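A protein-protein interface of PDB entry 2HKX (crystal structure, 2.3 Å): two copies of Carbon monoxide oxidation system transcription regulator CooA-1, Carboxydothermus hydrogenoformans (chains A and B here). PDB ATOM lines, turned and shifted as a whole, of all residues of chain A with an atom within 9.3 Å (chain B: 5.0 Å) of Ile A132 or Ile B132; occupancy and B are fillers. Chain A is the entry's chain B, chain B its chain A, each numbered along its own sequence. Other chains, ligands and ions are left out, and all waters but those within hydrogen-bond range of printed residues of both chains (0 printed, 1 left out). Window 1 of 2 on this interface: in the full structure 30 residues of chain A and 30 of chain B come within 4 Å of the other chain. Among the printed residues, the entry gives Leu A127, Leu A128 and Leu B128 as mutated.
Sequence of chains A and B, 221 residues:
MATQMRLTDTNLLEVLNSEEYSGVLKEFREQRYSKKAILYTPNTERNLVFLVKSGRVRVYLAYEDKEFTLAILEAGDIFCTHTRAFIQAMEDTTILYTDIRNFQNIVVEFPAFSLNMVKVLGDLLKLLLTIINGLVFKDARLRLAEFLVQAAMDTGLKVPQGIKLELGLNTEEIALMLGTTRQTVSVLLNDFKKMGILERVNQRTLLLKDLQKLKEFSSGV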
ATOM      1  N   VAL A  59     -25.313 -35.736  31.685  1.00  0.00           N
ATOM      2  CA  VAL A  59     -25.997 -34.435  31.765  1.00  0.00           C
ATOM      3  C   VAL A  59     -25.619 -33.699  30.463  1.00  0.00           C
ATOM      4  O   VAL A  59     -24.459 -33.592  30.148  1.00  0.00           O
ATOM      5  CB  VAL A  59     -25.508 -33.598  33.015  1.00  0.00           C
ATOM      6  CG1 VAL A  59     -26.223 -32.262  33.077  1.00  0.00           C
ATOM      7  CG2 VAL A  59     -25.727 -34.351  34.323  1.00  0.00           C
ATOM      8  N   TYR A  60     -26.609 -33.231  29.706  1.00  0.00           N
ATOM      9  CA  TYR A  60     -26.371 -32.649  28.386  1.00  0.00           C
ATOM     10  C   TYR A  60     -27.364 -31.531  28.074  1.00  0.00           C
ATOM     11  O   TYR A  60     -28.471 -31.515  28.601  1.00  0.00           O
ATOM     12  CB  TYR A  60     -26.344 -33.736  27.283  1.00  0.00           C
ATOM     13  CG  TYR A  60     -27.653 -34.463  27.021  1.00  0.00           C
ATOM     14  CD1 TYR A  60     -28.064 -35.528  27.838  1.00  0.00           C
ATOM     15  CD2 TYR A  60     -28.486 -34.072  25.969  1.00  0.00           C
ATOM     16  CE1 TYR A  60     -29.257 -36.185  27.625  1.00  0.00           C
ATOM     17  CE2 TYR A  60     -29.711 -34.734  25.725  1.00  0.00           C
ATOM     18  CZ  TYR A  60     -30.069 -35.795  26.557  1.00  0.00           C
ATOM     19  OH  TYR A  60     -31.262 -36.434  26.373  1.00  0.00           O
ATOM     20  N   LEU A  61     -26.941 -30.573  27.251  1.00  0.00           N
ATOM     21  CA  LEU A  61     -27.856 -29.577  26.690  1.00  0.00           C
ATOM     22  C   LEU A  61     -28.317 -30.053  25.333  1.00  0.00           C
ATOM     23  O   LEU A  61     -27.588 -30.734  24.643  1.00  0.00           O
ATOM     24  CB  LEU A  61     -27.151 -28.237  26.506  1.00  0.00           C
ATOM     25  CG  LEU A  61     -26.472 -27.633  27.717  1.00  0.00           C
ATOM     26  CD1 LEU A  61     -25.695 -26.459  27.265  1.00  0.00           C
ATOM     27  CD2 LEU A  61     -27.499 -27.289  28.778  1.00  0.00           C
ATOM     28  N   PHE A  68     -25.086 -31.198  23.466  1.00  0.00           N
ATOM     29  CA  PHE A  68     -23.795 -30.843  24.024  1.00  0.00           C
ATOM     30  C   PHE A  68     -23.729 -31.461  25.420  1.00  0.00           C
ATOM     31  O   PHE A  68     -24.485 -31.098  26.297  1.00  0.00           O
ATOM     32  CB  PHE A  68     -23.611 -29.320  24.065  1.00  0.00           C
ATOM     33  CG  PHE A  68     -22.208 -28.876  24.444  1.00  0.00           C
ATOM     34  CD1 PHE A  68     -21.219 -28.733  23.473  1.00  0.00           C
ATOM     35  CD2 PHE A  68     -21.881 -28.643  25.765  1.00  0.00           C
ATOM     36  CE1 PHE A  68     -19.917 -28.334  23.825  1.00  0.00           C
ATOM     37  CE2 PHE A  68     -20.593 -28.281  26.144  1.00  0.00           C
ATOM     38  CZ  PHE A  68     -19.605 -28.105  25.188  1.00  0.00           C
ATOM     39  N   THR A  69     -22.846 -32.432  25.589  1.00  0.00           N
ATOM     40  CA  THR A  69     -22.708 -33.146  26.856  1.00  0.00           C
ATOM     41  C   THR A  69     -21.871 -32.348  27.876  1.00  0.00           C
ATOM     42  O   THR A  69     -20.741 -31.960  27.591  1.00  0.00           O
ATOM     43  CB  THR A  69     -22.082 -34.551  26.617  1.00  0.00           C
ATOM     44  OG1 THR A  69     -23.036 -35.386  25.950  1.00  0.00           O
ATOM     45  CG2 THR A  69     -21.714 -35.219  27.931  1.00  0.00           C
ATOM     46  N   LEU A  70     -22.439 -32.117  29.052  1.00  0.00           N
ATOM     47  CA  LEU A  70     -21.762 -31.355  30.116  1.00  0.00           C
ATOM     48  C   LEU A  70     -20.914 -32.193  31.065  1.00  0.00           C
ATOM     49  O   LEU A  70     -19.840 -31.743  31.523  1.00  0.00           O
ATOM     50  CB  LEU A  70     -22.785 -30.570  30.956  1.00  0.00           C
ATOM     51  CG  LEU A  70     -23.629 -29.555  30.179  1.00  0.00           C
ATOM     52  CD1 LEU A  70     -24.857 -29.115  30.981  1.00  0.00           C
ATOM     53  CD2 LEU A  70     -22.840 -28.362  29.798  1.00  0.00           C
ATOM     54  N   ALA A  71     -21.387 -33.386  31.397  1.00  0.00           N
ATOM     55  CA  ALA A  71     -20.761 -34.166  32.466  1.00  0.00           C
ATOM     56  C   ALA A  71     -21.398 -35.530  32.553  1.00  0.00           C
ATOM     57  O   ALA A  71     -22.516 -35.712  32.131  1.00  0.00           O
ATOM     58  CB  ALA A  71     -20.939 -33.460  33.849  1.00  0.00           C
ATOM     59  N   ARG A  84     -31.293 -26.203  32.617  1.00  0.00           N
ATOM     60  CA  ARG A  84     -31.338 -26.356  31.162  1.00  0.00           C
ATOM     61  C   ARG A  84     -31.212 -27.804  30.691  1.00  0.00           C
ATOM     62  O   ARG A  84     -31.601 -28.111  29.565  1.00  0.00           O
ATOM     63  CB  ARG A  84     -30.200 -25.578  30.520  1.00  0.00           C
ATOM     64  CG  ARG A  84     -30.298 -24.119  30.695  1.00  0.00           C
ATOM     65  CD  ARG A  84     -31.679 -23.632  30.380  1.00  0.00           C
ATOM     66  NE  ARG A  84     -31.614 -22.709  29.264  1.00  0.00           N
ATOM     67  CZ  ARG A  84     -31.330 -21.425  29.403  1.00  0.00           C
ATOM     68  NH1 ARG A  84     -31.105 -20.919  30.614  1.00  0.00           N
ATOM     69  NH2 ARG A  84     -31.275 -20.655  28.334  1.00  0.00           N
ATOM     70  N   LEU A 124     -18.414 -30.642  40.211  1.00  0.00           N
ATOM     71  CA  LEU A 124     -19.208 -30.429  39.009  1.00  0.00           C
ATOM     72  C   LEU A 124     -19.004 -29.013  38.470  1.00  0.00           C
ATOM     73  O   LEU A 124     -18.898 -28.850  37.268  1.00  0.00           O
ATOM     74  CB  LEU A 124     -20.699 -30.795  39.189  1.00  0.00           C
ATOM     75  CG  LEU A 124     -21.707 -30.463  38.084  1.00  0.00           C
ATOM     76  CD1 LEU A 124     -21.233 -30.897  36.731  1.00  0.00           C
ATOM     77  CD2 LEU A 124     -23.083 -31.110  38.400  1.00  0.00           C
ATOM     78  N   LEU A 125     -18.948 -28.025  39.360  1.00  0.00           N
ATOM     79  CA  LEU A 125     -18.718 -26.617  39.023  1.00  0.00           C
ATOM     80  C   LEU A 125     -17.382 -26.429  38.379  1.00  0.00           C
ATOM     81  O   LEU A 125     -17.272 -25.675  37.443  1.00  0.00           O
ATOM     82  CB  LEU A 125     -18.761 -25.708  40.262  1.00  0.00           C
ATOM     83  CG  LEU A 125     -20.055 -25.782  41.054  1.00  0.00           C
ATOM     84  CD1 LEU A 125     -20.070 -24.832  42.288  1.00  0.00           C
ATOM     85  CD2 LEU A 125     -21.241 -25.501  40.121  1.00  0.00           C
ATOM     86  N   LYS A 126     -16.373 -27.131  38.877  1.00  0.00           N
ATOM     87  CA  LYS A 126     -15.027 -27.054  38.353  1.00  0.00           C
ATOM     88  C   LYS A 126     -15.118 -27.455  36.902  1.00  0.00           C
ATOM     89  O   LYS A 126     -14.657 -26.785  35.992  1.00  0.00           O
ATOM     90  CB  LYS A 126     -14.133 -28.039  39.105  1.00  0.00           C
ATOM     91  CG  LYS A 126     -12.757 -28.225  38.456  1.00  0.00           C
ATOM     92  CD  LYS A 126     -11.792 -28.979  39.340  1.00  0.00           C
ATOM     93  CE  LYS A 126     -10.401 -28.492  38.985  1.00  0.00           C
ATOM     94  NZ  LYS A 126      -9.346 -29.351  39.515  1.00  0.00           N
ATOM     95  N   LEU A 127     -15.759 -28.576  36.699  1.00  0.00           N
ATOM     96  CA  LEU A 127     -15.966 -29.145  35.404  1.00  0.00           C
ATOM     97  C   LEU A 127     -16.647 -28.188  34.434  1.00  0.00           C
ATOM     98  O   LEU A 127     -16.178 -27.997  33.310  1.00  0.00           O
ATOM     99  CB  LEU A 127     -16.790 -30.386  35.653  1.00  0.00           C
ATOM    100  CG  LEU A 127     -16.815 -31.533  34.700  1.00  0.00           C
ATOM    101  CD1 LEU A 127     -17.091 -32.848  35.467  1.00  0.00           C
ATOM    102  CD2 LEU A 127     -17.945 -31.196  33.752  1.00  0.00           C
ATOM    103  N   LEU A 128     -17.725 -27.552  34.879  1.00  0.00           N
ATOM    104  CA  LEU A 128     -18.468 -26.627  34.036  1.00  0.00           C
ATOM    105  C   LEU A 128     -17.655 -25.370  33.719  1.00  0.00           C
ATOM    106  O   LEU A 128     -17.796 -24.836  32.634  1.00  0.00           O
ATOM    107  CB  LEU A 128     -19.784 -26.235  34.704  1.00  0.00           C
ATOM    108  CG  LEU A 128     -20.794 -27.343  35.052  1.00  0.00           C
ATOM    109  CD1 LEU A 128     -21.895 -26.710  35.904  1.00  0.00           C
ATOM    110  CD2 LEU A 128     -21.361 -28.050  33.776  1.00  0.00           C
ATOM    111  N   LEU A 129     -16.806 -24.895  34.655  1.00  0.00           N
ATOM    112  CA  LEU A 129     -15.948 -23.743  34.393  1.00  0.00           C
ATOM    113  C   LEU A 129     -14.847 -24.053  33.373  1.00  0.00           C
ATOM    114  O   LEU A 129     -14.418 -23.177  32.597  1.00  0.00           O
ATOM    115  CB  LEU A 129     -15.327 -23.271  35.706  1.00  0.00           C
ATOM    116  CG  LEU A 129     -15.747 -21.953  36.346  1.00  0.00           C
ATOM    117  CD1 LEU A 129     -17.230 -21.658  36.230  1.00  0.00           C
ATOM    118  CD2 LEU A 129     -15.244 -21.797  37.803  1.00  0.00           C
ATOM    119  N   THR A 130     -14.335 -25.282  33.417  1.00  0.00           N
ATOM    120  CA  THR A 130     -13.426 -25.777  32.403  1.00  0.00           C
ATOM    121  C   THR A 130     -14.073 -25.737  30.994  1.00  0.00           C
ATOM    122  O   THR A 130     -13.423 -25.345  30.014  1.00  0.00           O
ATOM    123  CB  THR A 130     -12.988 -27.205  32.748  1.00  0.00           C
ATOM    124  OG1 THR A 130     -12.214 -27.163  33.939  1.00  0.00           O
ATOM    125  CG2 THR A 130     -12.149 -27.850  31.619  1.00  0.00           C
ATOM    126  N   ILE A 131     -15.339 -26.153  30.902  1.00  0.00           N
ATOM    127  CA  ILE A 131     -16.100 -26.021  29.652  1.00  0.00           C
ATOM    128  C   ILE A 131     -16.178 -24.551  29.200  1.00  0.00           C
ATOM    129  O   ILE A 131     -15.927 -24.251  28.013  1.00  0.00           O
ATOM    130  CB  ILE A 131     -17.533 -26.601  29.775  1.00  0.00           C
ATOM    131  CG1 ILE A 131     -17.492 -28.143  29.844  1.00  0.00           C
ATOM    132  CG2 ILE A 131     -18.409 -26.098  28.611  1.00  0.00           C
ATOM    133  CD1 ILE A 131     -18.802 -28.836  30.283  1.00  0.00           C
ATOM    134  N   ILE A 132     -16.566 -23.654  30.112  1.00  0.00           N
ATOM    135  CA  ILE A 132     -16.694 -22.243  29.790  1.00  0.00           C
ATOM    136  C   ILE A 132     -15.369 -21.672  29.254  1.00  0.00           C
ATOM    137  O   ILE A 132     -15.335 -21.116  28.175  1.00  0.00           O
ATOM    138  CB  ILE A 132     -17.230 -21.380  30.978  1.00  0.00           C
ATOM    139  CG1 ILE A 132     -18.663 -21.796  31.325  1.00  0.00           C
ATOM    140  CG2 ILE A 132     -17.194 -19.843  30.646  1.00  0.00           C
ATOM    141  CD1 ILE A 132     -19.174 -21.143  32.618  1.00  0.00           C
ATOM    142  N   ASN A 133     -14.295 -21.849  30.007  1.00  0.00           N
ATOM    143  CA  ASN A 133     -12.954 -21.503  29.591  1.00  0.00           C
ATOM    144  C   ASN A 133     -12.653 -21.984  28.151  1.00  0.00           C
ATOM    145  O   ASN A 133     -12.168 -21.210  27.298  1.00  0.00           O
ATOM    146  CB  ASN A 133     -12.012 -22.130  30.616  1.00  0.00           C
ATOM    147  CG  ASN A 133     -10.620 -21.571  30.575  1.00  0.00           C
ATOM    148  OD1 ASN A 133     -10.385 -20.424  30.944  1.00  0.00           O
ATOM    149  ND2 ASN A 133      -9.662 -22.407  30.168  1.00  0.00           N
ATOM    150  N   GLY A 134     -12.942 -23.260  27.883  1.00  0.00           N
ATOM    151  CA  GLY A 134     -12.670 -23.845  26.564  1.00  0.00           C
ATOM    152  C   GLY A 134     -13.478 -23.213  25.454  1.00  0.00           C
ATOM    153  O   GLY A 134     -12.978 -23.072  24.341  1.00  0.00           O
ATOM    154  N   LEU A 135     -14.730 -22.843  25.749  1.00  0.00           N
ATOM    155  CA  LEU A 135     -15.612 -22.155  24.784  1.00  0.00           C
ATOM    156  C   LEU A 135     -15.322 -20.667  24.563  1.00  0.00           C
ATOM    157  O   LEU A 135     -15.562 -20.167  23.483  1.00  0.00           O
ATOM    158  CB  LEU A 135     -17.097 -22.305  25.157  1.00  0.00           C
ATOM    159  CG  LEU A 135     -17.711 -23.708  25.151  1.00  0.00           C
ATOM    160  CD1 LEU A 135     -19.040 -23.729  25.912  1.00  0.00           C
ATOM    161  CD2 LEU A 135     -17.872 -24.218  23.736  1.00  0.00           C
ATOM    162  N   VAL A 136     -14.837 -19.945  25.567  1.00  0.00           N
ATOM    163  CA  VAL A 136     -14.737 -18.481  25.402  1.00  0.00           C
ATOM    164  C   VAL A 136     -13.375 -18.007  24.874  1.00  0.00           C
ATOM    165  O   VAL A 136     -13.257 -16.908  24.335  1.00  0.00           O
ATOM    166  CB  VAL A 136     -15.152 -17.688  26.690  1.00  0.00           C
ATOM    167  CG1 VAL A 136     -16.585 -18.059  27.137  1.00  0.00           C
ATOM    168  CG2 VAL A 136     -14.176 -17.919  27.826  1.00  0.00           C
ATOM    169  N   PHE A 137     -12.359 -18.843  25.028  1.00  0.00           N
ATOM    170  CA  PHE A 137     -11.010 -18.462  24.728  1.00  0.00           C
ATOM    171  C   PHE A 137     -10.439 -19.240  23.554  1.00  0.00           C
ATOM    172  O   PHE A 137      -9.229 -19.377  23.467  1.00  0.00           O
ATOM    173  CB  PHE A 137     -10.091 -18.689  25.949  1.00  0.00           C
ATOM    174  CG  PHE A 137     -10.390 -17.798  27.124  1.00  0.00           C
ATOM    175  CD1 PHE A 137     -10.534 -18.343  28.389  1.00  0.00           C
ATOM    176  CD2 PHE A 137     -10.511 -16.414  26.969  1.00  0.00           C
ATOM    177  CE1 PHE A 137     -10.818 -17.523  29.484  1.00  0.00           C
ATOM    178  CE2 PHE A 137     -10.788 -15.591  28.068  1.00  0.00           C
ATOM    179  CZ  PHE A 137     -10.938 -16.142  29.310  1.00  0.00           C
ATOM    180  N   LYS A 138     -11.270 -19.765  22.668  1.00  0.00           N
ATOM    181  CA  LYS A 138     -10.727 -20.357  21.469  1.00  0.00           C
ATOM    182  C   LYS A 138     -10.247 -19.280  20.505  1.00  0.00           C
ATOM    183  O   LYS A 138     -10.769 -18.159  20.495  1.00  0.00           O
ATOM    184  CB  LYS A 138     -11.623 -21.415  20.817  1.00  0.00           C
ATOM    185  CG  LYS A 138     -13.107 -21.190  20.816  1.00  0.00           C
ATOM    186  CD  LYS A 138     -13.741 -22.385  20.107  1.00  0.00           C
ATOM    187  CE  LYS A 138     -15.073 -22.769  20.731  1.00  0.00           C
ATOM    188  NZ  LYS A 138     -15.190 -24.255  20.765  1.00  0.00           N
ATOM    189  N   LEU B  61     -12.843 -15.092  34.275  1.00  0.00           N
ATOM    190  CA  LEU B  61     -11.777 -15.913  33.734  1.00  0.00           C
ATOM    191  C   LEU B  61     -10.887 -15.005  32.890  1.00  0.00           C
ATOM    192  O   LEU B  61     -11.421 -14.068  32.291  1.00  0.00           O
ATOM    193  CB  LEU B  61     -12.459 -16.909  32.826  1.00  0.00           C
ATOM    194  CG  LEU B  61     -12.920 -18.247  33.385  1.00  0.00           C
ATOM    195  CD1 LEU B  61     -12.926 -18.433  34.908  1.00  0.00           C
ATOM    196  CD2 LEU B  61     -14.131 -18.789  32.673  1.00  0.00           C
ATOM    197  N   PHE B  68     -13.479 -13.038  30.451  1.00  0.00           N
ATOM    198  CA  PHE B  68     -14.889 -13.352  30.354  1.00  0.00           C
ATOM    199  C   PHE B  68     -15.467 -13.243  31.766  1.00  0.00           C
ATOM    200  O   PHE B  68     -15.001 -13.905  32.672  1.00  0.00           O
ATOM    201  CB  PHE B  68     -15.085 -14.756  29.746  1.00  0.00           C
ATOM    202  CG  PHE B  68     -16.513 -15.166  29.650  1.00  0.00           C
ATOM    203  CD1 PHE B  68     -17.297 -14.775  28.557  1.00  0.00           C
ATOM    204  CD2 PHE B  68     -17.087 -15.954  30.647  1.00  0.00           C
ATOM    205  CE1 PHE B  68     -18.606 -15.130  28.465  1.00  0.00           C
ATOM    206  CE2 PHE B  68     -18.433 -16.321  30.560  1.00  0.00           C
ATOM    207  CZ  PHE B  68     -19.187 -15.908  29.481  1.00  0.00           C
ATOM    208  N   LEU B  70     -17.911 -13.990  34.619  1.00  0.00           N
ATOM    209  CA  LEU B  70     -18.848 -15.057  35.020  1.00  0.00           C
ATOM    210  C   LEU B  70     -19.984 -14.486  35.844  1.00  0.00           C
ATOM    211  O   LEU B  70     -21.141 -14.871  35.684  1.00  0.00           O
ATOM    212  CB  LEU B  70     -18.137 -16.146  35.851  1.00  0.00           C
ATOM    213  CG  LEU B  70     -17.015 -16.904  35.127  1.00  0.00           C
ATOM    214  CD1 LEU B  70     -16.102 -17.601  36.102  1.00  0.00           C
ATOM    215  CD2 LEU B  70     -17.561 -17.889  34.099  1.00  0.00           C
ATOM    216  N   LEU B 128     -24.313 -21.162  35.407  1.00  0.00           N
ATOM    217  CA  LEU B 128     -23.305 -21.800  34.535  1.00  0.00           C
ATOM    218  C   LEU B 128     -23.900 -22.636  33.391  1.00  0.00           C
ATOM    219  O   LEU B 128     -23.372 -22.583  32.291  1.00  0.00           O
ATOM    220  CB  LEU B 128     -22.304 -22.654  35.318  1.00  0.00           C
ATOM    221  CG  LEU B 128     -21.491 -21.896  36.385  1.00  0.00           C
ATOM    222  CD1 LEU B 128     -20.550 -22.870  37.097  1.00  0.00           C
ATOM    223  CD2 LEU B 128     -20.715 -20.688  35.805  1.00  0.00           C
ATOM    224  N   LEU B 129     -24.972 -23.406  33.635  1.00  0.00           N
ATOM    225  CA  LEU B 129     -25.568 -24.171  32.526  1.00  0.00           C
ATOM    226  C   LEU B 129     -26.105 -23.246  31.415  1.00  0.00           C
ATOM    227  O   LEU B 129     -26.011 -23.572  30.234  1.00  0.00           O
ATOM    228  CB  LEU B 129     -26.662 -25.115  32.995  1.00  0.00           C
ATOM    229  CG  LEU B 129     -26.356 -26.221  33.991  1.00  0.00           C
ATOM    230  CD1 LEU B 129     -27.598 -27.097  34.082  1.00  0.00           C
ATOM    231  CD2 LEU B 129     -25.153 -27.052  33.605  1.00  0.00           C
ATOM    232  N   THR B 130     -26.654 -22.104  31.840  1.00  0.00           N
ATOM    233  CA  THR B 130     -27.184 -21.032  31.013  1.00  0.00           C
ATOM    234  C   THR B 130     -26.097 -20.316  30.205  1.00  0.00           C
ATOM    235  O   THR B 130     -26.306 -19.988  29.053  1.00  0.00           O
ATOM    236  CB  THR B 130     -27.922 -19.969  31.917  1.00  0.00           C
ATOM    237  OG1 THR B 130     -29.078 -20.565  32.515  1.00  0.00           O
ATOM    238  CG2 THR B 130     -28.358 -18.749  31.115  1.00  0.00           C
ATOM    239  N   ILE B 131     -24.952 -20.044  30.810  1.00  0.00           N
ATOM    240  CA  ILE B 131     -23.833 -19.451  30.072  1.00  0.00           C
ATOM    241  C   ILE B 131     -23.408 -20.434  28.976  1.00  0.00           C
ATOM    242  O   ILE B 131     -23.355 -20.069  27.809  1.00  0.00           O
ATOM    243  CB  ILE B 131     -22.634 -19.122  31.021  1.00  0.00           C
ATOM    244  CG1 ILE B 131     -23.016 -17.991  31.998  1.00  0.00           C
ATOM    245  CG2 ILE B 131     -21.401 -18.721  30.229  1.00  0.00           C
ATOM    246  CD1 ILE B 131     -21.935 -17.682  33.074  1.00  0.00           C
ATOM    247  N   ILE B 132     -23.125 -21.691  29.360  1.00  0.00           N
ATOM    248  CA  ILE B 132     -22.700 -22.693  28.410  1.00  0.00           C
ATOM    249  C   ILE B 132     -23.682 -22.855  27.261  1.00  0.00           C
ATOM    250  O   ILE B 132     -23.283 -22.862  26.111  1.00  0.00           O
ATOM    251  CB  ILE B 132     -22.396 -24.052  29.075  1.00  0.00           C
ATOM    252  CG1 ILE B 132     -21.288 -23.847  30.121  1.00  0.00           C
ATOM    253  CG2 ILE B 132     -22.002 -25.093  27.993  1.00  0.00           C
ATOM    254  CD1 ILE B 132     -21.260 -24.954  31.183  1.00  0.00           C
ATOM    255  N   ASN B 133     -24.963 -22.951  27.577  1.00  0.00           N
ATOM    256  CA  ASN B 133     -26.004 -23.081  26.551  1.00  0.00           C
ATOM    257  C   ASN B 133     -25.969 -21.951  25.530  1.00  0.00           C
ATOM    258  O   ASN B 133     -26.072 -22.185  24.328  1.00  0.00           O
ATOM    259  CB  ASN B 133     -27.379 -23.159  27.214  1.00  0.00           C
ATOM    260  CG  ASN B 133     -28.496 -23.492  26.223  1.00  0.00           C
ATOM    261  OD1 ASN B 133     -28.614 -24.619  25.737  1.00  0.00           O
ATOM    262  ND2 ASN B 133     -29.328 -22.510  25.943  1.00  0.00           N
ATOM    263  N   GLY B 134     -25.842 -20.724  26.025  1.00  0.00           N
ATOM    264  CA  GLY B 134     -25.657 -19.565  25.176  1.00  0.00           C
ATOM    265  C   GLY B 134     -24.400 -19.678  24.335  1.00  0.00           C
ATOM    266  O   GLY B 134     -24.448 -19.439  23.167  1.00  0.00           O
ATOM    267  N   LEU B 135     -23.261 -20.008  24.933  1.00  0.00           N
ATOM    268  CA  LEU B 135     -22.028 -20.063  24.154  1.00  0.00           C
ATOM    269  C   LEU B 135     -22.098 -21.121  23.060  1.00  0.00           C
ATOM    270  O   LEU B 135     -21.582 -20.900  21.978  1.00  0.00           O
ATOM    271  CB  LEU B 135     -20.781 -20.252  25.043  1.00  0.00           C
ATOM    272  CG  LEU B 135     -20.511 -19.133  26.048  1.00  0.00           C
ATOM    273  CD1 LEU B 135     -19.571 -19.594  27.170  1.00  0.00           C
ATOM    274  CD2 LEU B 135     -19.987 -17.881  25.330  1.00  0.00           C
ATOM    275  N   VAL B 136     -22.771 -22.240  23.323  1.00  0.00           N
ATOM    276  CA  VAL B 136     -22.799 -23.353  22.366  1.00  0.00           C
ATOM    277  C   VAL B 136     -23.824 -23.184  21.243  1.00  0.00           C
ATOM    278  O   VAL B 136     -23.520 -23.437  20.075  1.00  0.00           O
ATOM    279  CB  VAL B 136     -22.895 -24.769  23.061  1.00  0.00           C
ATOM    280  CG1 VAL B 136     -21.818 -24.953  24.123  1.00  0.00           C
ATOM    281  CG2 VAL B 136     -24.212 -24.975  23.716  1.00  0.00           C
ATOM    282  N   PHE B 137     -25.031 -22.737  21.581  1.00  0.00           N
ATOM    283  CA  PHE B 137     -26.143 -22.773  20.631  1.00  0.00           C
ATOM    284  C   PHE B 137     -26.654 -21.396  20.205  1.00  0.00           C
ATOM    285  O   PHE B 137     -27.516 -21.325  19.355  1.00  0.00           O
ATOM    286  CB  PHE B 137     -27.329 -23.628  21.175  1.00  0.00           C
ATOM    287  CG  PHE B 137     -27.005 -25.106  21.344  1.00  0.00           C
ATOM    288  CD1 PHE B 137     -26.572 -25.877  20.252  1.00  0.00           C
ATOM    289  CD2 PHE B 137     -27.156 -25.731  22.579  1.00  0.00           C
ATOM    290  CE1 PHE B 137     -26.268 -27.246  20.405  1.00  0.00           C
ATOM    291  CE2 PHE B 137     -26.874 -27.118  22.748  1.00  0.00           C
ATOM    292  CZ  PHE B 137     -26.416 -27.869  21.661  1.00  0.00           C
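The side-chain hydroxyl (OG1) of Thr B130 is in hydrogen-bond range of the guanidinium group (NH1) of Arg A84 (2.8 Å).
The backbone NH of Leu A70 sits at hydrogen-bond distance from the backbone carbonyl oxygen of Val A59 (2.7 Å).
The backbone NH (N) of Leu A61 lies within hydrogen-bond range of the backbone carbonyl oxygen (O) of Phe A68.
The backbone NH of Leu B61 sits at hydrogen-bond distance from the backbone carbonyl oxygen of Phe B68, 2.9 Å away.
Among the printed residues, pairs that only touch across the chains: Leu A61 with Asn B133 (3.5 Å), Leu A61 with Phe B137 (3.9 Å), Phe A68 with Ile B132 (3.9 Å), Phe A68 with Val B136 (3.9 Å), Phe A68 with Phe B137 (3.97 Å), Leu A70 with Leu B129 (3.4 Å), Leu A70 with Ile B132 (3.8 Å), Arg A84 with Asn B133 (3.6 Å), Leu A128 with Leu B129 (3.9 Å), Leu A128 with Ile B132 (3.8 Å), Leu A129 with Leu B128 (3.6 Å), Ile A131 with Ile B132 (3.8 Å), Ile A132 with Leu B61 (3.8 Å), Ile A132 with Phe B68 (3.7 Å), Ile A132 with Leu B70 (3.9 Å), Ile A132 with Leu B128 (3.6 Å), Ile A132 with Ile B132 (3.5 Å), Leu A135 with Ile B132 (3.9 Å), Leu A135 with Leu B135 (3.98 Å), Leu A135 with Val B136 (3.5 Å), Val A136 with Phe B68 (3.6 Å), Val A136 with Leu B135 (3.4 Å) and Phe A137 with Leu B61 (3.7 Å).
Ile A132 touches just these residues of chain B: Leu B61 (3.8 Å), Phe B68 (3.7 Å), Leu B70 (3.9 Å), Leu B128 (3.6 Å) and Ile B132 (3.5 Å).
Of the printed residues of chain A, Ile B132 touches Phe A68, Leu A70, Leu A128, Ile A131, Ile A132 and Leu A135.
No residue of chain A comes within 4 Å of Gly B134.
Of the printed residues of chain B, Ile A131 touches Ile B132 (3.8 Å).
Of the printed residues of chain A, Leu B70 touches Ile A132 (3.9 Å).
Printed residues of chain B within 4 Å of Leu A129: Leu B128.
Ala A71 touches none of the printed residues of chain B.
The nearest residue of chain B that does not touch Ile A132 is Ile B131 (4.1 Å).
The nearest printed residue of chain A that does not touch Thr B130 is Leu A61 (6.1 Å).
Of the 23 printed residues of chain A, 11 touch a printed residue of chain B.
Hydrophobic or aromatic side chains of chain A that line the printed part of chain B: Leu A61, Phe A68, Leu A70, Leu A128, Leu A129, Ile A131, Ile A132, Leu A135, Val A136 and Phe A137.
Of the 13 printed residues of chain B, 11 touch a printed residue of chain A.
Phe A68 touches Ile B132, and with the chains exchanged Ile A132 touches Phe B68.
Leu A128 touches Leu B129, and with the chains exchanged Leu A129 touches Leu B128.
Leu A128 touches Ile B132, and with the chains exchanged Ile A132 touches Leu B128.
Leu B135 touches its own counterpart, Leu A135.
Positions printed for both chains: 61, 68, 70, 128, 129, 130, 131, 132, 133, 134, 135, 136 and 137.
Of the 24 pairs that touch across the chains among the printed residues, 16 have their exchanged pair printed and touching as well.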
